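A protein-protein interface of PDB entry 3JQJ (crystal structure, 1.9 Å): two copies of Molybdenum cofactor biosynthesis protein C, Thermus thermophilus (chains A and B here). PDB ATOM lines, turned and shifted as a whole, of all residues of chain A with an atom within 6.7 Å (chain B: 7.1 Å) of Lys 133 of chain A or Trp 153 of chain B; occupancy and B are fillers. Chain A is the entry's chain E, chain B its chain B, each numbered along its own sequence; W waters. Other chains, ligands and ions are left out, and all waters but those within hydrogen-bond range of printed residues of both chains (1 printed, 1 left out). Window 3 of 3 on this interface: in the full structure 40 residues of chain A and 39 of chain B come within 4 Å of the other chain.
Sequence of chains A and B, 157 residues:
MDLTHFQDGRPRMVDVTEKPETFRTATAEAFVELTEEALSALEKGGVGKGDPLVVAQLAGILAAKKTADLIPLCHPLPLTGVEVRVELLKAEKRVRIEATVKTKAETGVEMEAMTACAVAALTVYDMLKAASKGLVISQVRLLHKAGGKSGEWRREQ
The guanidinium group of Arg 155 of chain B is in hydrogen-bond range of the backbone carbonyl oxygen of Gly 134 of chain A (3.3 Å).
The side-chain sulfur of Met 114 of chain B is in hydrogen-bond range of the backbone NH of Leu 142 of chain B (3.5 Å). NE of Arg 155 of chain B is in hydrogen-bond range of O of Leu 142 of chain B. The backbone carbonyl oxygen of Leu 143 of chain B is in hydrogen-bond range of the backbone NH of Arg 155 of chain B, 2.9 Å away. N of Trp 153 of chain B is in hydrogen-bond range of O of Lys 145 of chain B (3.0 Å). OH of Tyr 125 of chain A lies within hydrogen-bond range of O of Lys 133 of chain A (2.9 Å).
Among the printed residues, merely in contact across the chains: Tyr 125 of chain A with Leu 142 of chain B, Val 136 of chain A with Arg 141 of chain B, Lys 133 of chain A with Leu 142 of chain B, Lys 133 of chain A with Trp 153 of chain B, Gly 134 of chain A with Trp 153 of chain B and Tyr 125 of chain A with Met 114 of chain B.
Of chain B, only Leu 142 and Trp 153 come within 4 Å of Lys 133 of chain A. Trp 153 of chain B touches just these residues of chain A: Lys 133 and Gly 134. Of the printed residues of chain B, Tyr 125 of chain A touches Met 114 and Leu 142. Of the printed residues of chain A, Arg 141 of chain B touches Val 136. Of the printed residues of chain A, Met 114 of chain B touches Tyr 125.
Of the 17 printed residues of chain B, 5 touch a printed residue of chain A. Hydrophobic or aromatic side chains of chain B within 4 Å of the printed part of chain A: Met 114, Leu 142 and Trp 153. Along chain B the printed residues that touch a printed residue of chain A span positions 114 to 155. Printed residues of chain A that touch a printed residue of chain B: Tyr 125, Lys 133, Gly 134 and Val 136. Among the printed residues, 7 pairs touch across the chains. Among the printed residues, no Asp or Glu carboxylate lies within 4 Å of a Lys or Arg side-chain nitrogen of the other chain.
No position is printed for both chains. Of the 7 pairs that touch across the chains among the printed residues, none has its exchanged pair printed and touching as well.
Water W1 bridges OE1 of Glu 110 of chain B (2.8 Å) and NZ of Lys 129 of chain A (3.4 Å).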
ATOM      1  N   TYR A 125      16.524  -9.285 -20.941  1.00  0.00           N
ATOM      2  CA  TYR A 125      16.141  -9.531 -19.555  1.00  0.00           C
ATOM      3  C   TYR A 125      14.698 -10.045 -19.507  1.00  0.00           C
ATOM      4  O   TYR A 125      14.390 -11.018 -18.819  1.00  0.00           O
ATOM      5  CB  TYR A 125      16.254  -8.233 -18.745  1.00  0.00           C
ATOM      6  CG  TYR A 125      15.798  -8.368 -17.316  1.00  0.00           C
ATOM      7  CD1 TYR A 125      16.626  -8.940 -16.349  1.00  0.00           C
ATOM      8  CD2 TYR A 125      14.526  -7.951 -16.934  1.00  0.00           C
ATOM      9  CE1 TYR A 125      16.194  -9.095 -15.033  1.00  0.00           C
ATOM     10  CE2 TYR A 125      14.082  -8.104 -15.623  1.00  0.00           C
ATOM     11  CZ  TYR A 125      14.918  -8.675 -14.678  1.00  0.00           C
ATOM     12  OH  TYR A 125      14.466  -8.849 -13.391  1.00  0.00           O
ATOM     13  N   LEU A 128      14.318 -13.626 -20.543  1.00  0.00           N
ATOM     14  CA  LEU A 128      14.950 -14.629 -19.686  1.00  0.00           C
ATOM     15  C   LEU A 128      14.699 -14.503 -18.182  1.00  0.00           C
ATOM     16  O   LEU A 128      15.021 -15.423 -17.428  1.00  0.00           O
ATOM     17  CB  LEU A 128      16.470 -14.637 -19.928  1.00  0.00           C
ATOM     18  CG  LEU A 128      16.978 -15.103 -21.299  1.00  0.00           C
ATOM     19  CD1 LEU A 128      18.476 -14.854 -21.413  1.00  0.00           C
ATOM     20  CD2 LEU A 128      16.670 -16.582 -21.487  1.00  0.00           C
ATOM     21  N   LYS A 129      14.121 -13.391 -17.735  1.00  0.00           N
ATOM     22  CA  LYS A 129      13.904 -13.213 -16.300  1.00  0.00           C
ATOM     23  C   LYS A 129      13.126 -14.344 -15.638  1.00  0.00           C
ATOM     24  O   LYS A 129      13.248 -14.566 -14.438  1.00  0.00           O
ATOM     25  CB  LYS A 129      13.227 -11.869 -16.007  1.00  0.00           C
ATOM     26  CG  LYS A 129      11.829 -11.702 -16.573  1.00  0.00           C
ATOM     27  CD  LYS A 129      11.279 -10.331 -16.204  1.00  0.00           C
ATOM     28  CE  LYS A 129       9.931 -10.070 -16.859  1.00  0.00           C
ATOM     29  NZ  LYS A 129       8.886 -11.019 -16.391  1.00  0.00           N
ATOM     30  N   ALA A 130      12.329 -15.062 -16.418  1.00  0.00           N
ATOM     31  CA  ALA A 130      11.564 -16.170 -15.866  1.00  0.00           C
ATOM     32  C   ALA A 130      12.544 -17.193 -15.294  1.00  0.00           C
ATOM     33  O   ALA A 130      12.232 -17.901 -14.339  1.00  0.00           O
ATOM     34  CB  ALA A 130      10.706 -16.806 -16.951  1.00  0.00           C
ATOM     35  N   ALA A 131      13.735 -17.256 -15.881  1.00  0.00           N
ATOM     36  CA  ALA A 131      14.767 -18.184 -15.429  1.00  0.00           C
ATOM     37  C   ALA A 131      15.538 -17.616 -14.237  1.00  0.00           C
ATOM     38  O   ALA A 131      15.855 -18.341 -13.293  1.00  0.00           O
ATOM     39  CB  ALA A 131      15.728 -18.494 -16.573  1.00  0.00           C
ATOM     40  N   SER A 132      15.837 -16.321 -14.288  1.00  0.00           N
ATOM     41  CA  SER A 132      16.577 -15.655 -13.219  1.00  0.00           C
ATOM     42  C   SER A 132      16.221 -14.174 -13.155  1.00  0.00           C
ATOM     43  O   SER A 132      16.476 -13.425 -14.097  1.00  0.00           O
ATOM     44  CB  SER A 132      18.083 -15.790 -13.452  1.00  0.00           C
ATOM     45  OG  SER A 132      18.464 -17.145 -13.584  1.00  0.00           O
ATOM     46  N   LYS A 133      15.647 -13.752 -12.035  1.00  0.00           N
ATOM     47  CA  LYS A 133      15.255 -12.358 -11.856  1.00  0.00           C
ATOM     48  C   LYS A 133      16.459 -11.461 -11.588  1.00  0.00           C
ATOM     49  O   LYS A 133      16.377 -10.242 -11.750  1.00  0.00           O
ATOM     50  CB  LYS A 133      14.261 -12.244 -10.696  1.00  0.00           C
ATOM     51  CG  LYS A 133      12.986 -13.043 -10.899  1.00  0.00           C
ATOM     52  CD  LYS A 133      12.599 -13.810  -9.641  1.00  0.00           C
ATOM     53  CE  LYS A 133      11.424 -14.738  -9.907  1.00  0.00           C
ATOM     54  NZ  LYS A 133      11.192 -15.684  -8.782  1.00  0.00           N
ATOM     55  N   GLY A 134      17.574 -12.074 -11.195  1.00  0.00           N
ATOM     56  CA  GLY A 134      18.777 -11.321 -10.881  1.00  0.00           C
ATOM     57  C   GLY A 134      19.688 -10.933 -12.033  1.00  0.00           C
ATOM     58  O   GLY A 134      20.758 -10.358 -11.808  1.00  0.00           O
ATOM     59  N   LEU A 135      19.279 -11.242 -13.259  1.00  0.00           N
ATOM     60  CA  LEU A 135      20.076 -10.905 -14.431  1.00  0.00           C
ATOM     61  C   LEU A 135      20.411  -9.421 -14.410  1.00  0.00           C
ATOM     62  O   LEU A 135      19.572  -8.592 -14.061  1.00  0.00           O
ATOM     63  CB  LEU A 135      19.308 -11.237 -15.709  1.00  0.00           C
ATOM     64  CG  LEU A 135      19.000 -12.716 -15.938  1.00  0.00           C
ATOM     65  CD1 LEU A 135      18.155 -12.872 -17.196  1.00  0.00           C
ATOM     66  CD2 LEU A 135      20.304 -13.494 -16.062  1.00  0.00           C
ATOM     67  N   VAL A 136      21.633  -9.083 -14.800  1.00  0.00           N
ATOM     68  CA  VAL A 136      22.047  -7.693 -14.789  1.00  0.00           C
ATOM     69  C   VAL A 136      22.512  -7.144 -16.130  1.00  0.00           C
ATOM     70  O   VAL A 136      23.188  -7.829 -16.898  1.00  0.00           O
ATOM     71  CB  VAL A 136      23.196  -7.475 -13.773  1.00  0.00           C
ATOM     72  CG1 VAL A 136      23.607  -6.008 -13.758  1.00  0.00           C
ATOM     73  CG2 VAL A 136      22.763  -7.929 -12.390  1.00  0.00           C
ATOM     74  N   THR B  27      11.083  -3.096  -7.748  1.00  0.00           N
ATOM     75  CA  THR B  27      12.046  -2.033  -7.539  1.00  0.00           C
ATOM     76  C   THR B  27      13.353  -2.404  -8.216  1.00  0.00           C
ATOM     77  O   THR B  27      13.841  -3.520  -8.067  1.00  0.00           O
ATOM     78  CB  THR B  27      12.306  -1.818  -6.032  1.00  0.00           C
ATOM     79  OG1 THR B  27      11.080  -1.448  -5.389  1.00  0.00           O
ATOM     80  CG2 THR B  27      13.341  -0.718  -5.813  1.00  0.00           C
ATOM     81  N   GLU B 110       8.256  -5.896 -13.146  1.00  0.00           N
ATOM     82  CA  GLU B 110       9.717  -5.830 -13.114  1.00  0.00           C
ATOM     83  C   GLU B 110      10.235  -5.067 -14.325  1.00  0.00           C
ATOM     84  O   GLU B 110      11.186  -4.291 -14.216  1.00  0.00           O
ATOM     85  CB  GLU B 110      10.337  -7.236 -13.105  1.00  0.00           C
ATOM     86  CG  GLU B 110       9.965  -8.071 -11.896  1.00  0.00           C
ATOM     87  CD  GLU B 110       8.781  -8.988 -12.155  1.00  0.00           C
ATOM     88  OE1 GLU B 110       7.902  -8.624 -12.962  1.00  0.00           O
ATOM     89  OE2 GLU B 110       8.728 -10.072 -11.537  1.00  0.00           O
ATOM     90  N   MET B 114      12.674  -1.767 -14.313  1.00  0.00           N
ATOM     91  CA  MET B 114      13.959  -1.828 -15.010  1.00  0.00           C
ATOM     92  C   MET B 114      14.055  -0.772 -16.112  1.00  0.00           C
ATOM     93  O   MET B 114      15.080  -0.099 -16.261  1.00  0.00           O
ATOM     94  CB  MET B 114      14.161  -3.222 -15.615  1.00  0.00           C
ATOM     95  CG  MET B 114      14.387  -4.327 -14.592  1.00  0.00           C
ATOM     96  SD  MET B 114      16.057  -4.268 -13.905  1.00  0.00           S
ATOM     97  CE  MET B 114      16.995  -5.009 -15.275  1.00  0.00           C
ATOM     98  N   ARG B 141      19.700  -3.230 -12.624  1.00  0.00           N
ATOM     99  CA  ARG B 141      19.295  -4.499 -12.026  1.00  0.00           C
ATOM    100  C   ARG B 141      18.097  -4.410 -11.087  1.00  0.00           C
ATOM    101  O   ARG B 141      17.808  -3.355 -10.524  1.00  0.00           O
ATOM    102  CB  ARG B 141      20.481  -5.072 -11.259  1.00  0.00           C
ATOM    103  CG  ARG B 141      20.926  -4.162 -10.127  1.00  0.00           C
ATOM    104  CD  ARG B 141      22.264  -4.575  -9.544  1.00  0.00           C
ATOM    105  NE  ARG B 141      22.579  -3.787  -8.355  1.00  0.00           N
ATOM    106  CZ  ARG B 141      23.737  -3.839  -7.705  1.00  0.00           C
ATOM    107  NH1 ARG B 141      24.705  -4.642  -8.130  1.00  0.00           N
ATOM    108  NH2 ARG B 141      23.921  -3.095  -6.624  1.00  0.00           N
ATOM    109  N   LEU B 142      17.423  -5.542 -10.902  1.00  0.00           N
ATOM    110  CA  LEU B 142      16.255  -5.615 -10.027  1.00  0.00           C
ATOM    111  C   LEU B 142      16.684  -5.786  -8.567  1.00  0.00           C
ATOM    112  O   LEU B 142      17.620  -6.532  -8.264  1.00  0.00           O
ATOM    113  CB  LEU B 142      15.357  -6.788 -10.432  1.00  0.00           C
ATOM    114  CG  LEU B 142      13.947  -6.780  -9.825  1.00  0.00           C
ATOM    115  CD1 LEU B 142      13.129  -5.667 -10.474  1.00  0.00           C
ATOM    116  CD2 LEU B 142      13.271  -8.117 -10.045  1.00  0.00           C
ATOM    117  N   LEU B 143      15.988  -5.095  -7.668  1.00  0.00           N
ATOM    118  CA  LEU B 143      16.293  -5.152  -6.245  1.00  0.00           C
ATOM    119  C   LEU B 143      15.202  -5.857  -5.449  1.00  0.00           C
ATOM    120  O   LEU B 143      15.480  -6.499  -4.435  1.00  0.00           O
ATOM    121  CB  LEU B 143      16.475  -3.737  -5.684  1.00  0.00           C
ATOM    122  CG  LEU B 143      17.596  -2.866  -6.259  1.00  0.00           C
ATOM    123  CD1 LEU B 143      17.540  -1.472  -5.630  1.00  0.00           C
ATOM    124  CD2 LEU B 143      18.936  -3.520  -5.988  1.00  0.00           C
ATOM    125  N   HIS B 144      13.961  -5.745  -5.911  1.00  0.00           N
ATOM    126  CA  HIS B 144      12.847  -6.356  -5.195  1.00  0.00           C
ATOM    127  C   HIS B 144      11.570  -6.440  -6.027  1.00  0.00           C
ATOM    128  O   HIS B 144      11.359  -5.657  -6.958  1.00  0.00           O
ATOM    129  CB  HIS B 144      12.585  -5.550  -3.912  1.00  0.00           C
ATOM    130  CG  HIS B 144      11.359  -5.966  -3.157  1.00  0.00           C
ATOM    131  ND1 HIS B 144      10.106  -5.458  -3.430  1.00  0.00           N
ATOM    132  CD2 HIS B 144      11.195  -6.839  -2.132  1.00  0.00           C
ATOM    133  CE1 HIS B 144       9.224  -6.001  -2.607  1.00  0.00           C
ATOM    134  NE2 HIS B 144       9.859  -6.842  -1.811  1.00  0.00           N
ATOM    135  N   LYS B 145      10.729  -7.412  -5.692  1.00  0.00           N
ATOM    136  CA  LYS B 145       9.451  -7.585  -6.360  1.00  0.00           C
ATOM    137  C   LYS B 145       8.558  -8.435  -5.456  1.00  0.00           C
ATOM    138  O   LYS B 145       9.044  -9.269  -4.687  1.00  0.00           O
ATOM    139  CB  LYS B 145       9.642  -8.227  -7.747  1.00  0.00           C
ATOM    140  CG  LYS B 145       9.666  -9.747  -7.798  1.00  0.00           C
ATOM    141  CD  LYS B 145       8.253 -10.302  -7.781  1.00  0.00           C
ATOM    142  CE  LYS B 145       8.229 -11.819  -7.798  1.00  0.00           C
ATOM    143  NZ  LYS B 145       6.825 -12.315  -7.688  1.00  0.00           N
ATOM    144  N   ALA B 146       7.254  -8.196  -5.521  1.00  0.00           N
ATOM    145  CA  ALA B 146       6.306  -8.945  -4.706  1.00  0.00           C
ATOM    146  C   ALA B 146       4.966  -9.005  -5.412  1.00  0.00           C
ATOM    147  O   ALA B 146       4.681  -8.196  -6.297  1.00  0.00           O
ATOM    148  CB  ALA B 146       6.149  -8.295  -3.340  1.00  0.00           C
ATOM    149  N   GLY B 147       4.141  -9.959  -5.000  1.00  0.00           N
ATOM    150  CA  GLY B 147       2.846 -10.128  -5.621  1.00  0.00           C
ATOM    151  C   GLY B 147       2.987 -11.248  -6.628  1.00  0.00           C
ATOM    152  O   GLY B 147       4.043 -11.415  -7.240  1.00  0.00           O
ATOM    153  N   SER B 150       4.956 -16.598  -7.298  1.00  0.00           N
ATOM    154  CA  SER B 150       6.338 -16.730  -6.849  1.00  0.00           C
ATOM    155  C   SER B 150       6.582 -16.084  -5.488  1.00  0.00           C
ATOM    156  O   SER B 150       7.485 -16.486  -4.757  1.00  0.00           O
ATOM    157  CB  SER B 150       7.294 -16.135  -7.888  1.00  0.00           C
ATOM    158  OG  SER B 150       6.966 -14.786  -8.166  1.00  0.00           O
ATOM    159  N   GLY B 151       5.778 -15.085  -5.142  1.00  0.00           N
ATOM    160  CA  GLY B 151       5.952 -14.433  -3.858  1.00  0.00           C
ATOM    161  C   GLY B 151       6.989 -13.328  -3.871  1.00  0.00           C
ATOM    162  O   GLY B 151       7.281 -12.739  -4.913  1.00  0.00           O
ATOM    163  N   GLU B 152       7.568 -13.051  -2.710  1.00  0.00           N
ATOM    164  CA  GLU B 152       8.556 -11.992  -2.602  1.00  0.00           C
ATOM    165  C   GLU B 152       9.974 -12.406  -2.995  1.00  0.00           C
ATOM    166  O   GLU B 152      10.382 -13.558  -2.818  1.00  0.00           O
ATOM    167  CB  GLU B 152       8.538 -11.435  -1.180  1.00  0.00           C
ATOM    168  CG  GLU B 152       9.322 -10.150  -1.009  1.00  0.00           C
ATOM    169  CD  GLU B 152       8.647  -9.188  -0.054  1.00  0.00           C
ATOM    170  OE1 GLU B 152       9.275  -8.175   0.310  1.00  0.00           O
ATOM    171  OE2 GLU B 152       7.481  -9.441   0.325  1.00  0.00           O
ATOM    172  N   TRP B 153      10.715 -11.447  -3.541  1.00  0.00           N
ATOM    173  CA  TRP B 153      12.091 -11.656  -3.971  1.00  0.00           C
ATOM    174  C   TRP B 153      12.868 -10.370  -3.702  1.00  0.00           C
ATOM    175  O   TRP B 153      12.351  -9.273  -3.911  1.00  0.00           O
ATOM    176  CB  TRP B 153      12.136 -11.971  -5.469  1.00  0.00           C
ATOM    177  CG  TRP B 153      13.519 -12.216  -6.010  1.00  0.00           C
ATOM    178  CD1 TRP B 153      14.164 -13.417  -6.101  1.00  0.00           C
ATOM    179  CD2 TRP B 153      14.423 -11.233  -6.532  1.00  0.00           C
ATOM    180  NE1 TRP B 153      15.413 -13.244  -6.653  1.00  0.00           N
ATOM    181  CE2 TRP B 153      15.598 -11.913  -6.925  1.00  0.00           C
ATOM    182  CE3 TRP B 153      14.355  -9.844  -6.705  1.00  0.00           C
ATOM    183  CZ2 TRP B 153      16.698 -11.250  -7.484  1.00  0.00           C
ATOM    184  CZ3 TRP B 153      15.445  -9.186  -7.259  1.00  0.00           C
ATOM    185  CH2 TRP B 153      16.603  -9.891  -7.642  1.00  0.00           C
ATOM    186  N   ARG B 154      14.105 -10.506  -3.236  1.00  0.00           N
ATOM    187  CA  ARG B 154      14.938  -9.346  -2.949  1.00  0.00           C
ATOM    188  C   ARG B 154      16.407  -9.678  -3.189  1.00  0.00           C
ATOM    189  O   ARG B 154      16.874 -10.754  -2.820  1.00  0.00           O
ATOM    190  CB  ARG B 154      14.735  -8.895  -1.496  1.00  0.00           C
ATOM    191  CG  ARG B 154      15.519  -7.643  -1.106  1.00  0.00           C
ATOM    192  CD  ARG B 154      15.136  -7.151   0.286  1.00  0.00           C
ATOM    193  NE  ARG B 154      15.465  -8.130   1.318  1.00  0.00           N
ATOM    194  CZ  ARG B 154      15.188  -7.989   2.613  1.00  0.00           C
ATOM    195  NH1 ARG B 154      14.569  -6.898   3.056  1.00  0.00           N
ATOM    196  NH2 ARG B 154      15.526  -8.947   3.466  1.00  0.00           N
ATOM    197  N   ARG B 155      17.128  -8.757  -3.820  1.00  0.00           N
ATOM    198  CA  ARG B 155      18.546  -8.959  -4.088  1.00  0.00           C
ATOM    199  C   ARG B 155      19.307  -8.822  -2.771  1.00  0.00           C
ATOM    200  O   ARG B 155      19.180  -7.815  -2.076  1.00  0.00           O
ATOM    201  CB  ARG B 155      19.054  -7.921  -5.095  1.00  0.00           C
ATOM    202  CG  ARG B 155      20.552  -7.990  -5.369  1.00  0.00           C
ATOM    203  CD  ARG B 155      20.973  -6.906  -6.345  1.00  0.00           C
ATOM    204  NE  ARG B 155      20.276  -7.056  -7.617  1.00  0.00           N
ATOM    205  CZ  ARG B 155      20.563  -7.985  -8.522  1.00  0.00           C
ATOM    206  NH1 ARG B 155      21.546  -8.849  -8.306  1.00  0.00           N
ATOM    207  NH2 ARG B 155      19.841  -8.074  -9.631  1.00  0.00           N
ATOM    208  N   GLU B 156      20.091  -9.840  -2.431  1.00  0.00           N
ATOM    209  CA  GLU B 156      20.861  -9.834  -1.191  1.00  0.00           C
ATOM    210  C   GLU B 156      22.361  -9.731  -1.457  1.00  0.00           C
ATOM    211  O   GLU B 156      23.149  -9.620  -0.518  1.00  0.00           O
ATOM    212  CB  GLU B 156      20.593 -11.116  -0.397  1.00  0.00           C
ATOM    213  CG  GLU B 156      19.142 -11.354  -0.002  1.00  0.00           C
ATOM    214  CD  GLU B 156      18.615 -10.325   0.979  1.00  0.00           C
ATOM    215  OE1 GLU B 156      19.376  -9.919   1.883  1.00  0.00           O
ATOM    216  OE2 GLU B 156      17.435  -9.934   0.857  1.00  0.00           O
HETATM  217  O   HOH W   1       6.188 -10.022 -14.597  1.00  0.00           O
